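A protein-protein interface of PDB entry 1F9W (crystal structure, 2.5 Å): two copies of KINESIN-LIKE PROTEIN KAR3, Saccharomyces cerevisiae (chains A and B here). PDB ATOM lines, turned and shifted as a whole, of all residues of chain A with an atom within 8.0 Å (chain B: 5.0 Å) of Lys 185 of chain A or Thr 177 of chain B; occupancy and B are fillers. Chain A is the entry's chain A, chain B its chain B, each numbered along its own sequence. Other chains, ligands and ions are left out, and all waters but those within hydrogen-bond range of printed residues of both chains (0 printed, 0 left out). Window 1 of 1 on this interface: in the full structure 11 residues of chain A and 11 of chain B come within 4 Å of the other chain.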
ATOM      1  N   PHE A 118      -9.679  27.939  -8.736  1.00  0.00           N
ATOM      2  CA  PHE A 118      -8.852  26.987  -8.024  1.00  0.00           C
ATOM      3  C   PHE A 118      -8.399  27.543  -6.697  1.00  0.00           C
ATOM      4  O   PHE A 118      -8.587  26.913  -5.664  1.00  0.00           O
ATOM      5  CB  PHE A 118      -7.641  26.630  -8.851  1.00  0.00           C
ATOM      6  CG  PHE A 118      -7.829  25.416  -9.702  1.00  0.00           C
ATOM      7  CD1 PHE A 118      -6.824  25.005 -10.574  1.00  0.00           C
ATOM      8  CD2 PHE A 118      -9.009  24.685  -9.652  1.00  0.00           C
ATOM      9  CE1 PHE A 118      -6.989  23.882 -11.393  1.00  0.00           C
ATOM     10  CE2 PHE A 118      -9.184  23.566 -10.464  1.00  0.00           C
ATOM     11  CZ  PHE A 118      -8.160  23.163 -11.341  1.00  0.00           C
ATOM     12  N   LYS A 132     -15.831  20.173  -6.247  1.00  0.00           N
ATOM     13  CA  LYS A 132     -15.564  19.191  -7.271  1.00  0.00           C
ATOM     14  C   LYS A 132     -15.595  20.021  -8.531  1.00  0.00           C
ATOM     15  O   LYS A 132     -16.397  20.929  -8.642  1.00  0.00           O
ATOM     16  CB  LYS A 132     -16.695  18.153  -7.298  1.00  0.00           C
ATOM     17  CG  LYS A 132     -16.246  16.709  -7.454  1.00  0.00           C
ATOM     18  CD  LYS A 132     -16.819  16.083  -8.733  1.00  0.00           C
ATOM     19  CE  LYS A 132     -15.871  16.257  -9.922  1.00  0.00           C
ATOM     20  NZ  LYS A 132     -16.437  15.676 -11.171  1.00  0.00           N
ATOM     21  N   VAL A 133     -14.716  19.742  -9.475  1.00  0.00           N
ATOM     22  CA  VAL A 133     -14.753  20.512 -10.694  1.00  0.00           C
ATOM     23  C   VAL A 133     -14.470  19.669 -11.908  1.00  0.00           C
ATOM     24  O   VAL A 133     -13.546  18.868 -11.940  1.00  0.00           O
ATOM     25  CB  VAL A 133     -13.783  21.707 -10.642  1.00  0.00           C
ATOM     26  CG1 VAL A 133     -13.497  22.238 -12.062  1.00  0.00           C
ATOM     27  CG2 VAL A 133     -14.397  22.817  -9.774  1.00  0.00           C
ATOM     28  N   ASN A 134     -15.324  19.843 -12.899  1.00  0.00           N
ATOM     29  CA  ASN A 134     -15.196  19.138 -14.150  1.00  0.00           C
ATOM     30  C   ASN A 134     -15.567  20.186 -15.174  1.00  0.00           C
ATOM     31  O   ASN A 134     -16.181  21.212 -14.859  1.00  0.00           O
ATOM     32  CB  ASN A 134     -16.161  17.951 -14.210  1.00  0.00           C
ATOM     33  CG  ASN A 134     -17.601  18.360 -13.944  1.00  0.00           C
ATOM     34  OD1 ASN A 134     -18.477  18.199 -14.803  1.00  0.00           O
ATOM     35  ND2 ASN A 134     -17.856  18.898 -12.751  1.00  0.00           N
ATOM     36  N   CYS A 135     -15.172  19.942 -16.404  1.00  0.00           N
ATOM     37  CA  CYS A 135     -15.477  20.880 -17.425  1.00  0.00           C
ATOM     38  C   CYS A 135     -15.651  20.124 -18.717  1.00  0.00           C
ATOM     39  O   CYS A 135     -15.489  18.902 -18.788  1.00  0.00           O
ATOM     40  CB  CYS A 135     -14.342  21.871 -17.559  1.00  0.00           C
ATOM     41  SG  CYS A 135     -12.931  21.198 -18.445  1.00  0.00           S
ATOM     42  N   GLU A 136     -16.003  20.881 -19.739  1.00  0.00           N
ATOM     43  CA  GLU A 136     -16.207  20.350 -21.063  1.00  0.00           C
ATOM     44  C   GLU A 136     -15.804  21.449 -22.019  1.00  0.00           C
ATOM     45  O   GLU A 136     -15.945  22.650 -21.726  1.00  0.00           O
ATOM     46  CB  GLU A 136     -17.689  19.991 -21.305  1.00  0.00           C
ATOM     47  CG  GLU A 136     -18.237  18.914 -20.384  1.00  0.00           C
ATOM     48  CD  GLU A 136     -18.963  19.516 -19.203  1.00  0.00           C
ATOM     49  OE1 GLU A 136     -19.455  20.659 -19.346  1.00  0.00           O
ATOM     50  OE2 GLU A 136     -19.038  18.864 -18.135  1.00  0.00           O
ATOM     51  N   LEU A 149     -12.810  18.096 -26.657  1.00  0.00           N
ATOM     52  CA  LEU A 149     -11.967  17.394 -25.691  1.00  0.00           C
ATOM     53  C   LEU A 149     -11.715  15.926 -26.018  1.00  0.00           C
ATOM     54  O   LEU A 149     -11.009  15.249 -25.274  1.00  0.00           O
ATOM     55  CB  LEU A 149     -12.552  17.514 -24.276  1.00  0.00           C
ATOM     56  CG  LEU A 149     -12.493  18.945 -23.715  1.00  0.00           C
ATOM     57  CD1 LEU A 149     -13.189  19.014 -22.370  1.00  0.00           C
ATOM     58  CD2 LEU A 149     -11.042  19.400 -23.593  1.00  0.00           C
ATOM     59  N   THR A 182     -17.404  14.776 -23.812  1.00  0.00           N
ATOM     60  CA  THR A 182     -16.339  14.563 -22.834  1.00  0.00           C
ATOM     61  C   THR A 182     -16.385  15.621 -21.759  1.00  0.00           C
ATOM     62  O   THR A 182     -16.417  16.813 -22.063  1.00  0.00           O
ATOM     63  CB  THR A 182     -14.927  14.651 -23.470  1.00  0.00           C
ATOM     64  OG1 THR A 182     -14.911  13.958 -24.726  1.00  0.00           O
ATOM     65  CG2 THR A 182     -13.880  14.050 -22.531  1.00  0.00           C
ATOM     66  N   SER A 183     -16.392  15.182 -20.511  1.00  0.00           N
ATOM     67  CA  SER A 183     -16.402  16.097 -19.373  1.00  0.00           C
ATOM     68  C   SER A 183     -15.193  15.727 -18.516  1.00  0.00           C
ATOM     69  O   SER A 183     -15.190  14.691 -17.846  1.00  0.00           O
ATOM     70  CB  SER A 183     -17.706  15.950 -18.567  1.00  0.00           C
ATOM     71  OG  SER A 183     -17.795  16.922 -17.529  1.00  0.00           O
ATOM     72  N   CYS A 184     -14.160  16.565 -18.556  1.00  0.00           N
ATOM     73  CA  CYS A 184     -12.921  16.311 -17.811  1.00  0.00           C
ATOM     74  C   CYS A 184     -12.939  16.822 -16.383  1.00  0.00           C
ATOM     75  O   CYS A 184     -13.310  17.967 -16.130  1.00  0.00           O
ATOM     76  CB  CYS A 184     -11.732  16.941 -18.532  1.00  0.00           C
ATOM     77  SG  CYS A 184     -11.102  15.988 -19.926  1.00  0.00           S
ATOM     78  N   LYS A 185     -12.539  15.963 -15.453  1.00  0.00           N
ATOM     79  CA  LYS A 185     -12.483  16.326 -14.040  1.00  0.00           C
ATOM     80  C   LYS A 185     -11.245  17.201 -13.888  1.00  0.00           C
ATOM     81  O   LYS A 185     -10.126  16.731 -14.111  1.00  0.00           O
ATOM     82  CB  LYS A 185     -12.321  15.075 -13.180  1.00  0.00           C
ATOM     83  CG  LYS A 185     -13.343  14.932 -12.092  1.00  0.00           C
ATOM     84  CD  LYS A 185     -13.252  13.533 -11.491  1.00  0.00           C
ATOM     85  CE  LYS A 185     -13.162  13.588  -9.954  1.00  0.00           C
ATOM     86  NZ  LYS A 185     -13.118  12.222  -9.324  1.00  0.00           N
ATOM     87  N   LEU A 186     -11.425  18.474 -13.552  1.00  0.00           N
ATOM     88  CA  LEU A 186     -10.272  19.342 -13.380  1.00  0.00           C
ATOM     89  C   LEU A 186      -9.764  19.008 -11.987  1.00  0.00           C
ATOM     90  O   LEU A 186     -10.058  19.699 -11.016  1.00  0.00           O
ATOM     91  CB  LEU A 186     -10.677  20.814 -13.499  1.00  0.00           C
ATOM     92  CG  LEU A 186     -11.046  21.277 -14.916  1.00  0.00           C
ATOM     93  CD1 LEU A 186     -11.523  22.705 -14.860  1.00  0.00           C
ATOM     94  CD2 LEU A 186      -9.863  21.138 -15.858  1.00  0.00           C
ATOM     95  N   GLU A 187      -9.009  17.914 -11.904  1.00  0.00           N
ATOM     96  CA  GLU A 187      -8.454  17.410 -10.642  1.00  0.00           C
ATOM     97  C   GLU A 187      -7.081  17.982 -10.274  1.00  0.00           C
ATOM     98  O   GLU A 187      -6.853  18.398  -9.138  1.00  0.00           O
ATOM     99  CB  GLU A 187      -8.372  15.884 -10.700  1.00  0.00           C
ATOM    100  CG  GLU A 187      -9.593  15.182 -10.143  1.00  0.00           C
ATOM    101  CD  GLU A 187      -9.467  13.665 -10.195  1.00  0.00           C
ATOM    102  OE1 GLU A 187      -8.762  13.145 -11.100  1.00  0.00           O
ATOM    103  OE2 GLU A 187     -10.073  12.993  -9.325  1.00  0.00           O
ATOM    104  N   SER A 188      -6.176  17.990 -11.248  1.00  0.00           N
ATOM    105  CA  SER A 188      -4.825  18.495 -11.073  1.00  0.00           C
ATOM    106  C   SER A 188      -4.558  19.649 -12.040  1.00  0.00           C
ATOM    107  O   SER A 188      -5.315  19.855 -12.987  1.00  0.00           O
ATOM    108  CB  SER A 188      -3.828  17.358 -11.319  1.00  0.00           C
ATOM    109  OG  SER A 188      -3.723  17.041 -12.701  1.00  0.00           O
ATOM    110  N   GLU A 189      -3.489  20.406 -11.806  1.00  0.00           N
ATOM    111  CA  GLU A 189      -3.171  21.514 -12.697  1.00  0.00           C
ATOM    112  C   GLU A 189      -2.482  20.942 -13.916  1.00  0.00           C
ATOM    113  O   GLU A 189      -2.302  21.621 -14.921  1.00  0.00           O
ATOM    114  CB  GLU A 189      -2.263  22.550 -12.014  1.00  0.00           C
ATOM    115  CG  GLU A 189      -3.019  23.673 -11.245  1.00  0.00           C
ATOM    116  CD  GLU A 189      -3.397  24.899 -12.105  1.00  0.00           C
ATOM    117  OE1 GLU A 189      -2.949  24.985 -13.270  1.00  0.00           O
ATOM    118  OE2 GLU A 189      -4.143  25.781 -11.607  1.00  0.00           O
ATOM    119  N   MET A 191      -3.699  18.523 -15.651  1.00  0.00           N
ATOM    120  CA  MET A 191      -4.830  18.372 -16.553  1.00  0.00           C
ATOM    121  C   MET A 191      -5.159  19.712 -17.185  1.00  0.00           C
ATOM    122  O   MET A 191      -5.155  19.855 -18.403  1.00  0.00           O
ATOM    123  CB  MET A 191      -6.038  17.857 -15.769  1.00  0.00           C
ATOM    124  CG  MET A 191      -7.283  17.568 -16.598  1.00  0.00           C
ATOM    125  SD  MET A 191      -7.048  16.169 -17.691  1.00  0.00           S
ATOM    126  CE  MET A 191      -6.368  16.980 -19.137  1.00  0.00           C
ATOM    127  N   VAL A 192      -5.457  20.683 -16.330  1.00  0.00           N
ATOM    128  CA  VAL A 192      -5.780  22.047 -16.743  1.00  0.00           C
ATOM    129  C   VAL A 192      -4.756  22.472 -17.779  1.00  0.00           C
ATOM    130  O   VAL A 192      -5.067  23.140 -18.761  1.00  0.00           O
ATOM    131  CB  VAL A 192      -5.685  23.008 -15.534  1.00  0.00           C
ATOM    132  CG1 VAL A 192      -5.916  24.419 -15.975  1.00  0.00           C
ATOM    133  CG2 VAL A 192      -6.696  22.623 -14.469  1.00  0.00           C
ATOM    134  N   ILE A 195      -5.488  20.292 -21.105  1.00  0.00           N
ATOM    135  CA  ILE A 195      -6.725  20.784 -21.658  1.00  0.00           C
ATOM    136  C   ILE A 195      -6.439  22.159 -22.243  1.00  0.00           C
ATOM    137  O   ILE A 195      -6.574  22.364 -23.450  1.00  0.00           O
ATOM    138  CB  ILE A 195      -7.817  20.850 -20.542  1.00  0.00           C
ATOM    139  CG1 ILE A 195      -8.308  19.439 -20.227  1.00  0.00           C
ATOM    140  CG2 ILE A 195      -9.016  21.697 -20.975  1.00  0.00           C
ATOM    141  CD1 ILE A 195      -9.087  19.360 -18.945  1.00  0.00           C
ATOM    142  N   GLU B 166      -2.883   8.322  -9.837  1.00  0.00           N
ATOM    143  CA  GLU B 166      -2.656   7.682  -8.568  1.00  0.00           C
ATOM    144  C   GLU B 166      -3.989   7.304  -7.970  1.00  0.00           C
ATOM    145  O   GLU B 166      -4.953   8.079  -7.988  1.00  0.00           O
ATOM    146  CB  GLU B 166      -1.889   8.621  -7.627  1.00  0.00           C
ATOM    147  CG  GLU B 166      -1.177   9.783  -8.317  1.00  0.00           C
ATOM    148  CD  GLU B 166      -1.274  11.059  -7.507  1.00  0.00           C
ATOM    149  OE1 GLU B 166      -1.229  12.158  -8.109  1.00  0.00           O
ATOM    150  OE2 GLU B 166      -1.403  10.952  -6.265  1.00  0.00           O
ATOM    151  N   ILE B 167      -4.043   6.099  -7.438  1.00  0.00           N
ATOM    152  CA  ILE B 167      -5.267   5.636  -6.829  1.00  0.00           C
ATOM    153  C   ILE B 167      -5.565   6.493  -5.610  1.00  0.00           C
ATOM    154  O   ILE B 167      -4.795   6.509  -4.648  1.00  0.00           O
ATOM    155  CB  ILE B 167      -5.118   4.174  -6.404  1.00  0.00           C
ATOM    156  CG1 ILE B 167      -4.918   3.312  -7.648  1.00  0.00           C
ATOM    157  CG2 ILE B 167      -6.320   3.743  -5.584  1.00  0.00           C
ATOM    158  CD1 ILE B 167      -3.924   2.221  -7.461  1.00  0.00           C
ATOM    159  N   ARG B 168      -6.674   7.213  -5.640  1.00  0.00           N
ATOM    160  CA  ARG B 168      -7.002   8.036  -4.498  1.00  0.00           C
ATOM    161  C   ARG B 168      -8.285   7.588  -3.816  1.00  0.00           C
ATOM    162  O   ARG B 168      -9.388   7.807  -4.318  1.00  0.00           O
ATOM    163  CB  ARG B 168      -7.077   9.494  -4.925  1.00  0.00           C
ATOM    164  CG  ARG B 168      -5.719  10.034  -5.354  1.00  0.00           C
ATOM    165  CD  ARG B 168      -5.031  10.822  -4.232  1.00  0.00           C
ATOM    166  NE  ARG B 168      -5.467  12.217  -4.222  1.00  0.00           N
ATOM    167  CZ  ARG B 168      -4.891  13.190  -4.924  1.00  0.00           C
ATOM    168  NH1 ARG B 168      -3.845  12.925  -5.692  1.00  0.00           N
ATOM    169  NH2 ARG B 168      -5.377  14.423  -4.878  1.00  0.00           N
ATOM    170  N   HIS B 169      -8.121   6.965  -2.654  1.00  0.00           N
ATOM    171  CA  HIS B 169      -9.231   6.452  -1.870  1.00  0.00           C
ATOM    172  C   HIS B 169      -9.980   7.460  -1.032  1.00  0.00           C
ATOM    173  O   HIS B 169      -9.458   8.519  -0.684  1.00  0.00           O
ATOM    174  CB  HIS B 169      -8.737   5.359  -0.937  1.00  0.00           C
ATOM    175  CG  HIS B 169      -8.274   4.135  -1.647  1.00  0.00           C
ATOM    176  ND1 HIS B 169      -9.138   3.273  -2.275  1.00  0.00           N
ATOM    177  CD2 HIS B 169      -7.033   3.645  -1.854  1.00  0.00           C
ATOM    178  CE1 HIS B 169      -8.452   2.304  -2.841  1.00  0.00           C
ATOM    179  NE2 HIS B 169      -7.171   2.503  -2.601  1.00  0.00           N
ATOM    180  N   THR B 175     -15.260   5.037  -1.602  1.00  0.00           N
ATOM    181  CA  THR B 175     -15.072   5.119  -3.039  1.00  0.00           C
ATOM    182  C   THR B 175     -13.578   5.060  -3.386  1.00  0.00           C
ATOM    183  O   THR B 175     -12.766   4.748  -2.516  1.00  0.00           O
ATOM    184  CB  THR B 175     -15.735   6.398  -3.610  1.00  0.00           C
ATOM    185  OG1 THR B 175     -15.223   7.559  -2.950  1.00  0.00           O
ATOM    186  CG2 THR B 175     -17.243   6.337  -3.390  1.00  0.00           C
ATOM    187  N   THR B 176     -13.230   5.345  -4.644  1.00  0.00           N
ATOM    188  CA  THR B 176     -11.840   5.294  -5.120  1.00  0.00           C
ATOM    189  C   THR B 176     -11.742   5.915  -6.497  1.00  0.00           C
ATOM    190  O   THR B 176     -12.290   5.395  -7.467  1.00  0.00           O
ATOM    191  CB  THR B 176     -11.322   3.840  -5.261  1.00  0.00           C
ATOM    192  OG1 THR B 176     -11.202   3.243  -3.964  1.00  0.00           O
ATOM    193  CG2 THR B 176      -9.962   3.799  -5.981  1.00  0.00           C
ATOM    194  N   THR B 177     -11.038   7.028  -6.590  1.00  0.00           N
ATOM    195  CA  THR B 177     -10.867   7.678  -7.869  1.00  0.00           C
ATOM    196  C   THR B 177      -9.485   7.318  -8.359  1.00  0.00           C
ATOM    197  O   THR B 177      -8.755   6.575  -7.709  1.00  0.00           O
ATOM    198  CB  THR B 177     -10.910   9.199  -7.737  1.00  0.00           C
ATOM    199  OG1 THR B 177     -11.906   9.574  -6.776  1.00  0.00           O
ATOM    200  CG2 THR B 177     -11.216   9.838  -9.078  1.00  0.00           C
ATOM    201  N   ILE B 178      -9.135   7.853  -9.511  1.00  0.00           N
ATOM    202  CA  ILE B 178      -7.827   7.642 -10.076  1.00  0.00           C
ATOM    203  C   ILE B 178      -7.605   8.951 -10.785  1.00  0.00           C
ATOM    204  O   ILE B 178      -8.350   9.338 -11.688  1.00  0.00           O
ATOM    205  CB  ILE B 178      -7.809   6.457 -11.027  1.00  0.00           C
ATOM    206  CG1 ILE B 178      -7.961   5.162 -10.217  1.00  0.00           C
ATOM    207  CG2 ILE B 178      -6.483   6.419 -11.775  1.00  0.00           C
ATOM    208  CD1 ILE B 178      -8.664   4.012 -10.928  1.00  0.00           C
ATOM    209  N   THR B 179      -6.596   9.665 -10.330  1.00  0.00           N
ATOM    210  CA  THR B 179      -6.307  10.972 -10.867  1.00  0.00           C
ATOM    211  C   THR B 179      -6.108  11.042 -12.374  1.00  0.00           C
ATOM    212  O   THR B 179      -5.506  10.160 -12.983  1.00  0.00           O
ATOM    213  CB  THR B 179      -5.100  11.554 -10.130  1.00  0.00           C
ATOM    214  OG1 THR B 179      -3.903  10.872 -10.527  1.00  0.00           O
ATOM    215  CG2 THR B 179      -5.295  11.352  -8.627  1.00  0.00           C
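Among the printed residues, no Asp or Glu carboxylate lies within 4 Å of a Lys or Arg side-chain nitrogen of the other chain.
OE2 of Glu 187 of chain A lies within salt-bridge range of NZ of Lys 185 of chain A (3.1 Å).
The side-chain hydroxyl (OG1) of Thr 179 of chain B is in hydrogen-bond range of the backbone NH (N) of Glu 166 of chain B (2.8 Å).
The backbone carbonyl oxygen of Arg 168 of chain B is in hydrogen-bond range of the backbone NH of Thr 177 of chain B, at 2.9 Å.
Among the printed residues, merely in contact across the chains: Lys 185 of chain A with Thr 177 of chain B (3.1 Å), Glu 187 of chain A with Thr 179 of chain B (3.3 Å), Glu 187 of chain A with Thr 177 of chain B (3.4 Å) and Glu 187 of chain A with Ile 178 of chain B (3.9 Å).
No position is printed for both chains.
Lys 185 of chain A touches one residue of chain B.
Of chain A, only Lys 185 and Glu 187 come within 4 Å of Thr 177 of chain B.
Of the printed residues of chain A, Thr 179 of chain B touches Glu 187 (3.3 Å).
Printed residues of chain B within 4 Å of Glu 187 of chain A: Thr 177, Ile 178 and Thr 179.
Of the printed residues of chain A, Ile 178 of chain B touches Glu 187 (3.9 Å).
Thr 175 of chain B touches none of the printed residues of chain A.
The nearest printed residue of chain B that does not touch Lys 185 of chain A is Ile 178 of chain B (5.9 Å).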
